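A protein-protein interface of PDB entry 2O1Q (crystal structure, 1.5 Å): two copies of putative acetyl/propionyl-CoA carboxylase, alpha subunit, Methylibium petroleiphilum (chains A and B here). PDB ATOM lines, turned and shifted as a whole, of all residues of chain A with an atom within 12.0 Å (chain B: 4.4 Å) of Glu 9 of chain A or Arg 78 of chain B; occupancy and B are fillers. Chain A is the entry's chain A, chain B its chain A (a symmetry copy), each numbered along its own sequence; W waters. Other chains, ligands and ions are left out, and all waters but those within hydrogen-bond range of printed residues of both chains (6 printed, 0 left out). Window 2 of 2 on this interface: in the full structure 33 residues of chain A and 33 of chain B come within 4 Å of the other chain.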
ATOM      1  N   SER A   5      36.018  -4.263 -29.072  1.00  0.00           N
ATOM      2  CA  SER A   5      34.825  -5.007 -28.666  1.00  0.00           C
ATOM      3  C   SER A   5      33.543  -4.382 -29.114  1.00  0.00           C
ATOM      4  O   SER A   5      33.499  -3.196 -29.471  1.00  0.00           O
ATOM      5  CB  SER A   5      34.787  -5.137 -27.155  1.00  0.00           C
ATOM      6  OG  SER A   5      34.977  -3.896 -26.506  1.00  0.00           O
ATOM      7  N   LYS A   6      32.469  -5.179 -29.083  1.00  0.00           N
ATOM      8  CA  LYS A   6      31.167  -4.644 -29.412  1.00  0.00           C
ATOM      9  C   LYS A   6      30.696  -3.726 -28.291  1.00  0.00           C
ATOM     10  O   LYS A   6      31.186  -3.788 -27.147  1.00  0.00           O
ATOM     11  CB  LYS A   6      30.166  -5.737 -29.662  1.00  0.00           C
ATOM     12  CG  LYS A   6      29.840  -6.587 -28.481  1.00  0.00           C
ATOM     13  CD  LYS A   6      29.073  -7.814 -28.931  1.00  0.00           C
ATOM     14  CE  LYS A   6      28.219  -8.397 -27.821  1.00  0.00           C
ATOM     15  NZ  LYS A   6      26.965  -7.613 -27.517  1.00  0.00           N
ATOM     16  N   ILE A   7      29.813  -2.818 -28.666  1.00  0.00           N
ATOM     17  CA  ILE A   7      29.205  -1.859 -27.735  1.00  0.00           C
ATOM     18  C   ILE A   7      28.226  -2.586 -26.815  1.00  0.00           C
ATOM     19  O   ILE A   7      27.490  -3.434 -27.228  1.00  0.00           O
ATOM     20  CB  ILE A   7      28.635  -0.634 -28.456  1.00  0.00           C
ATOM     21  CG1 ILE A   7      29.746  -0.006 -29.325  1.00  0.00           C
ATOM     22  CG2 ILE A   7      28.022   0.336 -27.434  1.00  0.00           C
ATOM     23  CD1 ILE A   7      30.910   0.533 -28.581  1.00  0.00           C
ATOM     24  N   LYS A   8      28.252  -2.196 -25.555  1.00  0.00           N
ATOM     25  CA  LYS A   8      27.318  -2.714 -24.546  1.00  0.00           C
ATOM     26  C   LYS A   8      25.884  -2.256 -24.834  1.00  0.00           C
ATOM     27  O   LYS A   8      25.646  -1.121 -25.231  1.00  0.00           O
ATOM     28  CB  LYS A   8      27.744  -2.214 -23.168  1.00  0.00           C
ATOM     29  CG  LYS A   8      28.981  -2.898 -22.559  1.00  0.00           C
ATOM     30  N   GLU A   9      24.931  -3.156 -24.619  1.00  0.00           N
ATOM     31  CA  GLU A   9      23.539  -2.764 -24.615  1.00  0.00           C
ATOM     32  C   GLU A   9      23.236  -2.045 -23.320  1.00  0.00           C
ATOM     33  O   GLU A   9      23.912  -2.206 -22.289  1.00  0.00           O
ATOM     34  CB  GLU A   9      22.602  -3.968 -24.804  1.00  0.00           C
ATOM     35  CG  GLU A   9      22.936  -4.864 -26.052  1.00  0.00           C
ATOM     36  CD  GLU A   9      23.884  -6.009 -25.775  1.00  0.00           C
ATOM     37  OE1 GLU A   9      24.435  -6.069 -24.655  1.00  0.00           O
ATOM     38  OE2 GLU A   9      24.091  -6.880 -26.660  1.00  0.00           O
ATOM     39  N   GLU A  10      22.203  -1.233 -23.396  1.00  0.00           N
ATOM     40  CA  GLU A  10      21.753  -0.385 -22.300  1.00  0.00           C
ATOM     41  C   GLU A  10      20.262  -0.518 -22.069  1.00  0.00           C
ATOM     42  O   GLU A  10      19.498  -0.817 -22.982  1.00  0.00           O
ATOM     43  CB  GLU A  10      22.047   1.081 -22.580  1.00  0.00           C
ATOM     44  CG  GLU A  10      23.478   1.363 -22.958  1.00  0.00           C
ATOM     45  CD  GLU A  10      23.690   2.762 -23.521  1.00  0.00           C
ATOM     46  OE1 GLU A  10      22.788   3.644 -23.459  1.00  0.00           O
ATOM     47  OE2 GLU A  10      24.789   2.986 -24.046  1.00  0.00           O
ATOM     48  N   TYR A  11      19.873  -0.301 -20.825  1.00  0.00           N
ATOM     49  CA  TYR A  11      18.473  -0.259 -20.408  1.00  0.00           C
ATOM     50  C   TYR A  11      18.295   0.830 -19.362  1.00  0.00           C
ATOM     51  O   TYR A  11      19.113   0.938 -18.447  1.00  0.00           O
ATOM     52  CB  TYR A  11      17.973  -1.589 -19.857  1.00  0.00           C
ATOM     53  CG  TYR A  11      16.544  -1.476 -19.407  1.00  0.00           C
ATOM     54  CD1 TYR A  11      15.520  -1.247 -20.330  1.00  0.00           C
ATOM     55  CD2 TYR A  11      16.219  -1.482 -18.079  1.00  0.00           C
ATOM     56  CE1 TYR A  11      14.235  -1.051 -19.938  1.00  0.00           C
ATOM     57  CE2 TYR A  11      14.943  -1.282 -17.659  1.00  0.00           C
ATOM     58  CZ  TYR A  11      13.954  -1.072 -18.609  1.00  0.00           C
ATOM     59  OH  TYR A  11      12.679  -0.858 -18.198  1.00  0.00           O
ATOM     60  N   VAL A  12      17.254   1.638 -19.506  1.00  0.00           N
ATOM     61  CA  VAL A  12      16.922   2.687 -18.569  1.00  0.00           C
ATOM     62  C   VAL A  12      15.473   2.513 -18.127  1.00  0.00           C
ATOM     63  O   VAL A  12      14.568   2.559 -18.990  1.00  0.00           O
ATOM     64  CB  VAL A  12      17.051   4.131 -19.185  1.00  0.00           C
ATOM     65  CG1 VAL A  12      16.515   5.214 -18.208  1.00  0.00           C
ATOM     66  CG2 VAL A  12      18.472   4.383 -19.630  1.00  0.00           C
ATOM     67  N   GLN A  13      15.260   2.365 -16.828  1.00  0.00           N
ATOM     68  CA  GLN A  13      13.924   2.360 -16.273  1.00  0.00           C
ATOM     69  C   GLN A  13      13.491   3.808 -16.049  1.00  0.00           C
ATOM     70  O   GLN A  13      13.913   4.470 -15.126  1.00  0.00           O
ATOM     71  CB  GLN A  13      13.945   1.564 -14.974  1.00  0.00           C
ATOM     72  CG  GLN A  13      12.596   1.273 -14.366  1.00  0.00           C
ATOM     73  CD  GLN A  13      11.732   0.486 -15.336  1.00  0.00           C
ATOM     74  OE1 GLN A  13      12.125  -0.603 -15.749  1.00  0.00           O
ATOM     75  NE2 GLN A  13      10.598   1.053 -15.746  1.00  0.00           N
ATOM     76  N   LEU A  36      18.348   9.953 -22.219  1.00  0.00           N
ATOM     77  CA  LEU A  36      18.207   8.507 -22.203  1.00  0.00           C
ATOM     78  C   LEU A  36      19.450   7.804 -22.733  1.00  0.00           C
ATOM     79  O   LEU A  36      19.838   6.721 -22.242  1.00  0.00           O
ATOM     80  CB  LEU A  36      17.004   8.109 -23.015  1.00  0.00           C
ATOM     81  CG  LEU A  36      15.654   8.598 -22.467  1.00  0.00           C
ATOM     82  CD1 LEU A  36      14.548   8.266 -23.500  1.00  0.00           C
ATOM     83  CD2 LEU A  36      15.367   8.054 -21.054  1.00  0.00           C
ATOM     84  N   HIS A  37      20.124   8.433 -23.686  1.00  0.00           N
ATOM     85  CA  HIS A  37      21.266   7.772 -24.333  1.00  0.00           C
ATOM     86  C   HIS A  37      22.118   8.775 -25.080  1.00  0.00           C
ATOM     87  O   HIS A  37      21.590   9.718 -25.712  1.00  0.00           O
ATOM     88  CB  HIS A  37      20.800   6.662 -25.287  1.00  0.00           C
ATOM     89  CG  HIS A  37      21.894   6.085 -26.134  1.00  0.00           C
ATOM     90  ND1 HIS A  37      22.739   5.095 -25.693  1.00  0.00           N
ATOM     91  CD2 HIS A  37      22.268   6.366 -27.395  1.00  0.00           C
ATOM     92  CE1 HIS A  37      23.628   4.833 -26.639  1.00  0.00           C
ATOM     93  NE2 HIS A  37      23.342   5.573 -27.695  1.00  0.00           N
ATOM     94  N   VAL A  38      23.416   8.566 -25.083  1.00  0.00           N
ATOM     95  CA  VAL A  38      24.314   9.217 -26.018  1.00  0.00           C
ATOM     96  C   VAL A  38      25.182   8.156 -26.707  1.00  0.00           C
ATOM     97  O   VAL A  38      25.634   7.227 -26.011  1.00  0.00           O
ATOM     98  CB  VAL A  38      25.178  10.336 -25.384  1.00  0.00           C
ATOM     99  CG1 VAL A  38      24.295  11.449 -24.767  1.00  0.00           C
ATOM    100  CG2 VAL A  38      26.248   9.754 -24.416  1.00  0.00           C
ATOM    101  N   SER A  39      25.504   8.378 -27.975  1.00  0.00           N
ATOM    102  CA  SER A  39      26.360   7.560 -28.798  1.00  0.00           C
ATOM    103  C   SER A  39      27.583   8.398 -29.158  1.00  0.00           C
ATOM    104  O   SER A  39      27.508   9.255 -30.075  1.00  0.00           O
ATOM    105  CB  SER A  39      25.663   7.176 -30.072  1.00  0.00           C
ATOM    106  OG  SER A  39      24.769   6.077 -29.846  1.00  0.00           O
ATOM    107  N   PRO A  40      28.686   8.201 -28.445  1.00  0.00           N
ATOM    108  CA  PRO A  40      29.867   9.039 -28.703  1.00  0.00           C
ATOM    109  C   PRO A  40      30.479   8.899 -30.079  1.00  0.00           C
ATOM    110  O   PRO A  40      31.195   9.832 -30.563  1.00  0.00           O
ATOM    111  CB  PRO A  40      30.881   8.553 -27.636  1.00  0.00           C
ATOM    112  CG  PRO A  40      30.074   7.858 -26.618  1.00  0.00           C
ATOM    113  CD  PRO A  40      28.968   7.200 -27.399  1.00  0.00           C
ATOM    114  N   VAL B  77      14.311  -9.028 -23.270  1.00  0.00           N
ATOM    115  CA  VAL B  77      15.336  -8.916 -24.317  1.00  0.00           C
ATOM    116  C   VAL B  77      16.616  -9.611 -23.842  1.00  0.00           C
ATOM    117  O   VAL B  77      16.966  -9.568 -22.668  1.00  0.00           O
ATOM    118  CB  VAL B  77      15.641  -7.439 -24.674  1.00  0.00           C
ATOM    119  CG1 VAL B  77      16.187  -7.347 -26.103  1.00  0.00           C
ATOM    120  CG2 VAL B  77      14.400  -6.543 -24.499  1.00  0.00           C
ATOM    121  N   ARG B  78      17.307 -10.253 -24.775  1.00  0.00           N
ATOM    122  CA  ARG B  78      18.518 -11.010 -24.480  1.00  0.00           C
ATOM    123  C   ARG B  78      18.341 -11.988 -23.320  1.00  0.00           C
ATOM    124  O   ARG B  78      19.281 -12.193 -22.519  1.00  0.00           O
ATOM    125  CB  ARG B  78      19.708 -10.056 -24.277  1.00  0.00           C
ATOM    126  CG  ARG B  78      20.148  -9.416 -25.570  1.00  0.00           C
ATOM    127  CD  ARG B  78      21.145  -8.263 -25.421  1.00  0.00           C
ATOM    128  NE  ARG B  78      20.433  -7.059 -24.940  1.00  0.00           N
ATOM    129  CZ  ARG B  78      20.462  -6.603 -23.700  1.00  0.00           C
ATOM    130  NH1 ARG B  78      21.142  -7.217 -22.754  1.00  0.00           N
ATOM    131  NH2 ARG B  78      19.776  -5.528 -23.389  1.00  0.00           N
ATOM    132  N   GLY B  79      17.151 -12.599 -23.212  1.00  0.00           N
ATOM    133  CA  GLY B  79      16.849 -13.502 -22.105  1.00  0.00           C
ATOM    134  C   GLY B  79      16.121 -12.948 -20.878  1.00  0.00           C
ATOM    135  O   GLY B  79      15.538 -13.707 -20.099  1.00  0.00           O
ATOM    136  N   GLY B  80      16.066 -11.636 -20.727  1.00  0.00           N
ATOM    137  CA  GLY B  80      15.422 -11.058 -19.586  1.00  0.00           C
ATOM    138  C   GLY B  80      16.444 -10.852 -18.512  1.00  0.00           C
ATOM    139  O   GLY B  80      17.548 -11.410 -18.563  1.00  0.00           O
ATOM    140  N   GLY B  84      20.382 -12.484 -17.488  1.00  0.00           N
ATOM    141  CA  GLY B  84      21.538 -11.652 -17.789  1.00  0.00           C
ATOM    142  C   GLY B  84      21.313 -10.708 -18.950  1.00  0.00           C
ATOM    143  O   GLY B  84      22.230  -9.955 -19.339  1.00  0.00           O
ATOM    144  N   GLY B  85      20.108 -10.735 -19.518  1.00  0.00           N
ATOM    145  CA  GLY B  85      19.673  -9.656 -20.409  1.00  0.00           C
ATOM    146  C   GLY B  85      18.943  -8.576 -19.640  1.00  0.00           C
ATOM    147  O   GLY B  85      19.299  -8.224 -18.502  1.00  0.00           O
ATOM    148  N   ASP B  86      17.878  -8.062 -20.235  1.00  0.00           N
ATOM    149  CA  ASP B  86      17.073  -7.030 -19.592  1.00  0.00           C
ATOM    150  C   ASP B  86      15.589  -7.357 -19.684  1.00  0.00           C
ATOM    151  O   ASP B  86      15.103  -8.011 -20.636  1.00  0.00           O
ATOM    152  CB  ASP B  86      17.384  -5.644 -20.198  1.00  0.00           C
ATOM    153  CG  ASP B  86      18.722  -5.082 -19.709  1.00  0.00           C
ATOM    154  OD1 ASP B  86      18.818  -4.815 -18.484  1.00  0.00           O
ATOM    155  OD2 ASP B  86      19.644  -4.872 -20.535  1.00  0.00           O
ATOM    156  N   TYR B  95      18.951   0.526 -25.542  1.00  0.00           N
ATOM    157  CA  TYR B  95      19.885   0.688 -26.657  1.00  0.00           C
ATOM    158  C   TYR B  95      20.385  -0.701 -26.945  1.00  0.00           C
ATOM    159  O   TYR B  95      21.037  -1.305 -26.063  1.00  0.00           O
ATOM    160  CB  TYR B  95      21.049   1.562 -26.227  1.00  0.00           C
ATOM    161  CG  TYR B  95      22.080   1.803 -27.305  1.00  0.00           C
ATOM    162  CD1 TYR B  95      21.816   2.630 -28.391  1.00  0.00           C
ATOM    163  CD2 TYR B  95      23.296   1.147 -27.273  1.00  0.00           C
ATOM    164  CE1 TYR B  95      22.745   2.816 -29.408  1.00  0.00           C
ATOM    165  CE2 TYR B  95      24.247   1.371 -28.236  1.00  0.00           C
ATOM    166  CZ  TYR B  95      23.947   2.176 -29.328  1.00  0.00           C
ATOM    167  OH  TYR B  95      24.922   2.435 -30.292  1.00  0.00           O
ATOM    168  N   GLU B  96      20.051  -1.200 -28.135  1.00  0.00           N
ATOM    169  CA  GLU B  96      20.479  -2.524 -28.586  1.00  0.00           C
ATOM    170  C   GLU B  96      21.569  -2.290 -29.622  1.00  0.00           C
ATOM    171  O   GLU B  96      21.294  -1.820 -30.702  1.00  0.00           O
ATOM    172  CB  GLU B  96      19.266  -3.334 -29.057  1.00  0.00           C
ATOM    173  CG  GLU B  96      18.224  -3.631 -27.843  1.00  0.00           C
ATOM    174  CD  GLU B  96      18.763  -4.513 -26.643  1.00  0.00           C
ATOM    175  OE1 GLU B  96      19.450  -5.503 -27.055  1.00  0.00           O
ATOM    176  OE2 GLU B  96      18.619  -4.324 -25.310  1.00  0.00           O
ATOM    177  N   SER B  97      22.830  -2.541 -29.243  1.00  0.00           N
ATOM    178  CA  SER B  97      23.998  -2.156 -30.048  1.00  0.00           C
ATOM    179  C   SER B  97      24.136  -3.009 -31.302  1.00  0.00           C
ATOM    180  O   SER B  97      23.524  -4.094 -31.444  1.00  0.00           O
ATOM    181  CB  SER B  97      25.238  -2.270 -29.201  1.00  0.00           C
ATOM    182  OG  SER B  97      25.255  -3.477 -28.443  1.00  0.00           O
ATOM    183  N   ALA B 100      23.972  -6.955 -31.582  1.00  0.00           N
ATOM    184  CA  ALA B 100      23.129  -7.578 -30.558  1.00  0.00           C
ATOM    185  C   ALA B 100      22.358  -8.781 -31.094  1.00  0.00           C
ATOM    186  O   ALA B 100      21.730  -8.690 -32.142  1.00  0.00           O
ATOM    187  CB  ALA B 100      22.107  -6.549 -29.939  1.00  0.00           C
ATOM    188  N   ARG B 101      22.383  -9.887 -30.343  1.00  0.00           N
ATOM    189  CA  ARG B 101      21.666 -11.121 -30.713  1.00  0.00           C
ATOM    190  C   ARG B 101      20.434 -11.279 -29.859  1.00  0.00           C
ATOM    191  O   ARG B 101      20.513 -11.319 -28.621  1.00  0.00           O
ATOM    192  CB  ARG B 101      22.508 -12.357 -30.441  1.00  0.00           C
ATOM    193  CG  ARG B 101      23.828 -12.380 -31.156  1.00  0.00           C
ATOM    194  N   HIS B 102      19.305 -11.343 -30.549  1.00  0.00           N
ATOM    195  CA  HIS B 102      17.975 -11.365 -29.934  1.00  0.00           C
ATOM    196  C   HIS B 102      17.328 -12.711 -30.284  1.00  0.00           C
ATOM    197  O   HIS B 102      16.603 -12.796 -31.290  1.00  0.00           O
ATOM    198  CB  HIS B 102      17.112 -10.196 -30.525  1.00  0.00           C
ATOM    199  CG  HIS B 102      17.467  -8.808 -30.015  1.00  0.00           C
ATOM    200  ND1 HIS B 102      16.960  -7.587 -30.552  1.00  0.00           N
ATOM    201  CD2 HIS B 102      18.325  -8.488 -29.028  1.00  0.00           C
ATOM    202  CE1 HIS B 102      17.465  -6.619 -29.804  1.00  0.00           C
ATOM    203  NE2 HIS B 102      18.313  -7.127 -28.919  1.00  0.00           N
HETATM  204  O   HOH W   1      24.147   4.497 -31.979  1.00  0.00           O
HETATM  205  O   HOH W   2      23.879  -9.589 -27.688  1.00  0.00           O
HETATM  206  O   HOH W   3      17.690  -2.827 -23.630  1.00  0.00           O
HETATM  207  O   HOH W   4      26.865   4.066 -28.136  1.00  0.00           O
HETATM  208  O   HOH W   5      26.190  -5.832 -29.292  1.00  0.00           O
HETATM  209  O   HOH W   6      21.695  -3.429 -20.015  1.00  0.00           O
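Tyr 95 of chain B touches Ile 7 of chain A (CE2 to CG2, 3.996 Å). Tyr 95 of chain B touches Lys 8 of chain A. Ser 97 of chain B touches Lys 8 of chain A (OG to C, 3.9 Å). Glu 9 of chain A touches Tyr 95 of chain B. Glu 9 of chain A touches Glu 96 of chain B (CG to OE1, 3.7 Å). Glu 9 of chain A touches Ser 97 of chain B. CB of Ala 100 of chain B touches OE2 of Glu 9 of chain A, at 3.8 Å. Tyr 11 of chain A touches Asp 86 of chain B (CB to CG, 3.6 Å). His 37 of chain A touches Tyr 95 of chain B (NE2 to CE1, 3.3 Å). OH of Tyr 95 of chain B touches OG of Ser 39 of chain A, 3.7 Å away.
No position is printed for both chains.
Of the 13 printed residues of chain B, 6 touch a printed residue of chain A. Printed residues of chain B that touch a printed residue of chain A: Arg 78, Asp 86, Tyr 95, Glu 96, Ser 97 and Ala 100. Hydrophobic or aromatic side chains of chain B that line the printed part of chain A: Tyr 95 and Ala 100. Of the 14 printed residues of chain A, 7 touch a printed residue of chain B. Hydrophobic or aromatic side chains of chain A within 4 Å of the printed part of chain B: Ile 7, Tyr 11 and His 37. Among the printed residues, Asp or Glu carboxylates within 4 Å of a Lys or Arg side-chain nitrogen of the other chain: Glu 9 of chain A with Arg 78 of chain B (3.97 Å).
Water W3 lies within hydrogen-bond range of the side-chain carboxylate of Glu 96 of chain B (2.4 Å), the backbone carbonyl oxygen of Glu 10 of chain A (2.8 Å) and the guanidinium group of Arg 78 of chain B (3.4 Å). Water W6 lies within hydrogen-bond range of OD2 of Asp 86 of chain B (2.6 Å) and O of Glu 9 of chain A (3.4 Å). Water W5 lies within hydrogen-bond range of NZ of Lys 6 of chain A (2.6 Å), OG of Ser 97 of chain B (2.7 Å), N of Ala 100 of chain B (3.4 Å) and O of Ile 7 of chain A (3.4 Å). Water W1 lies within hydrogen-bond range of the side-chain hydroxyl of Ser 39 of chain A and the side-chain hydroxyl of Tyr 95 of chain B. Water W2 lies within hydrogen-bond range of the side-chain carboxylate (OE2) of Glu 9 of chain A (2.9 Å) and the backbone NH (N) of Arg 101 of chain B (3.1 Å). Water W4 bridges OH of Tyr 95 of chain B and OG of Ser 39 of chain A.
The backbone carbonyl oxygen of Tyr 95 of chain B sits at hydrogen-bond distance from the backbone NH of Glu 10 of chain A (2.9 Å). NH1 of Arg 78 of chain B is in salt-bridge range of OE1 of Glu 9 of chain A, 3.97 Å away. OG of Ser 97 of chain B sits at hydrogen-bond distance from O of Ile 7 of chain A (2.5 Å).
Printed residues of chain B within 4 Å of Glu 9 of chain A: Arg 78 (3.5 Å), Tyr 95 (3.2 Å), Glu 96 (3.7 Å), Ser 97 (3.6 Å) and Ala 100 (3.8 Å). Arg 78 of chain B touches just one residue of chain A: Glu 9. No residue of chain A comes within 4 Å of Gly 79 of chain B. Gly 80 of chain B touches none of the printed residues of chain A. No residue of chain A comes within 4 Å of Gly 84 of chain B. Of chain A, only Glu 9 (3.7 Å) comes within 4 Å of Glu 96 of chain B. No residue of chain A comes within 4 Å of Arg 101 of chain B. No residue of chain A comes within 4 Å of His 102 of chain B. Of the printed residues of chain A, Tyr 95 of chain B touches Ile 7, Lys 8, Glu 9, Glu 10, His 37 and Ser 39. Of the printed residues of chain B, Lys 8 of chain A touches Tyr 95 (3.9 Å) and Ser 97 (3.9 Å). Printed residues of chain A within 4 Å of Ser 97 of chain B: Ile 7, Lys 8 and Glu 9. Val 77 of chain B touches none of the printed residues of chain A. Lys 6 of chain A touches none of the printed residues of chain B. The nearest residue of chain A that does not touch Arg 78 of chain B is Glu 10 of chain A (4.7 Å).
The side-chain hydroxyl (OH) of Tyr 11 of chain A lies within hydrogen-bond range of the side-chain amide oxygen (OE1) of Gln 13 of chain A, 2.5 Å away. NZ of Lys 6 of chain A is in salt-bridge range of OE2 of Glu 9 of chain A (3.1 Å). The side-chain carboxylate (OD2) of Asp 86 of chain B is in salt-bridge range of the guanidinium group (NH2) of Arg 78 of chain B, at 2.9 Å. OE1 of Glu 96 of chain B lies within hydrogen-bond range of NE2 of His 102 of chain B. NE2 of His 37 of chain A is in hydrogen-bond range of OG of Ser 39 of chain A, 2.6 Å away. The backbone NH (N) of Val 77 of chain B lies within hydrogen-bond range of the backbone carbonyl oxygen (O) of Asp 86 of chain B (2.9 Å).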
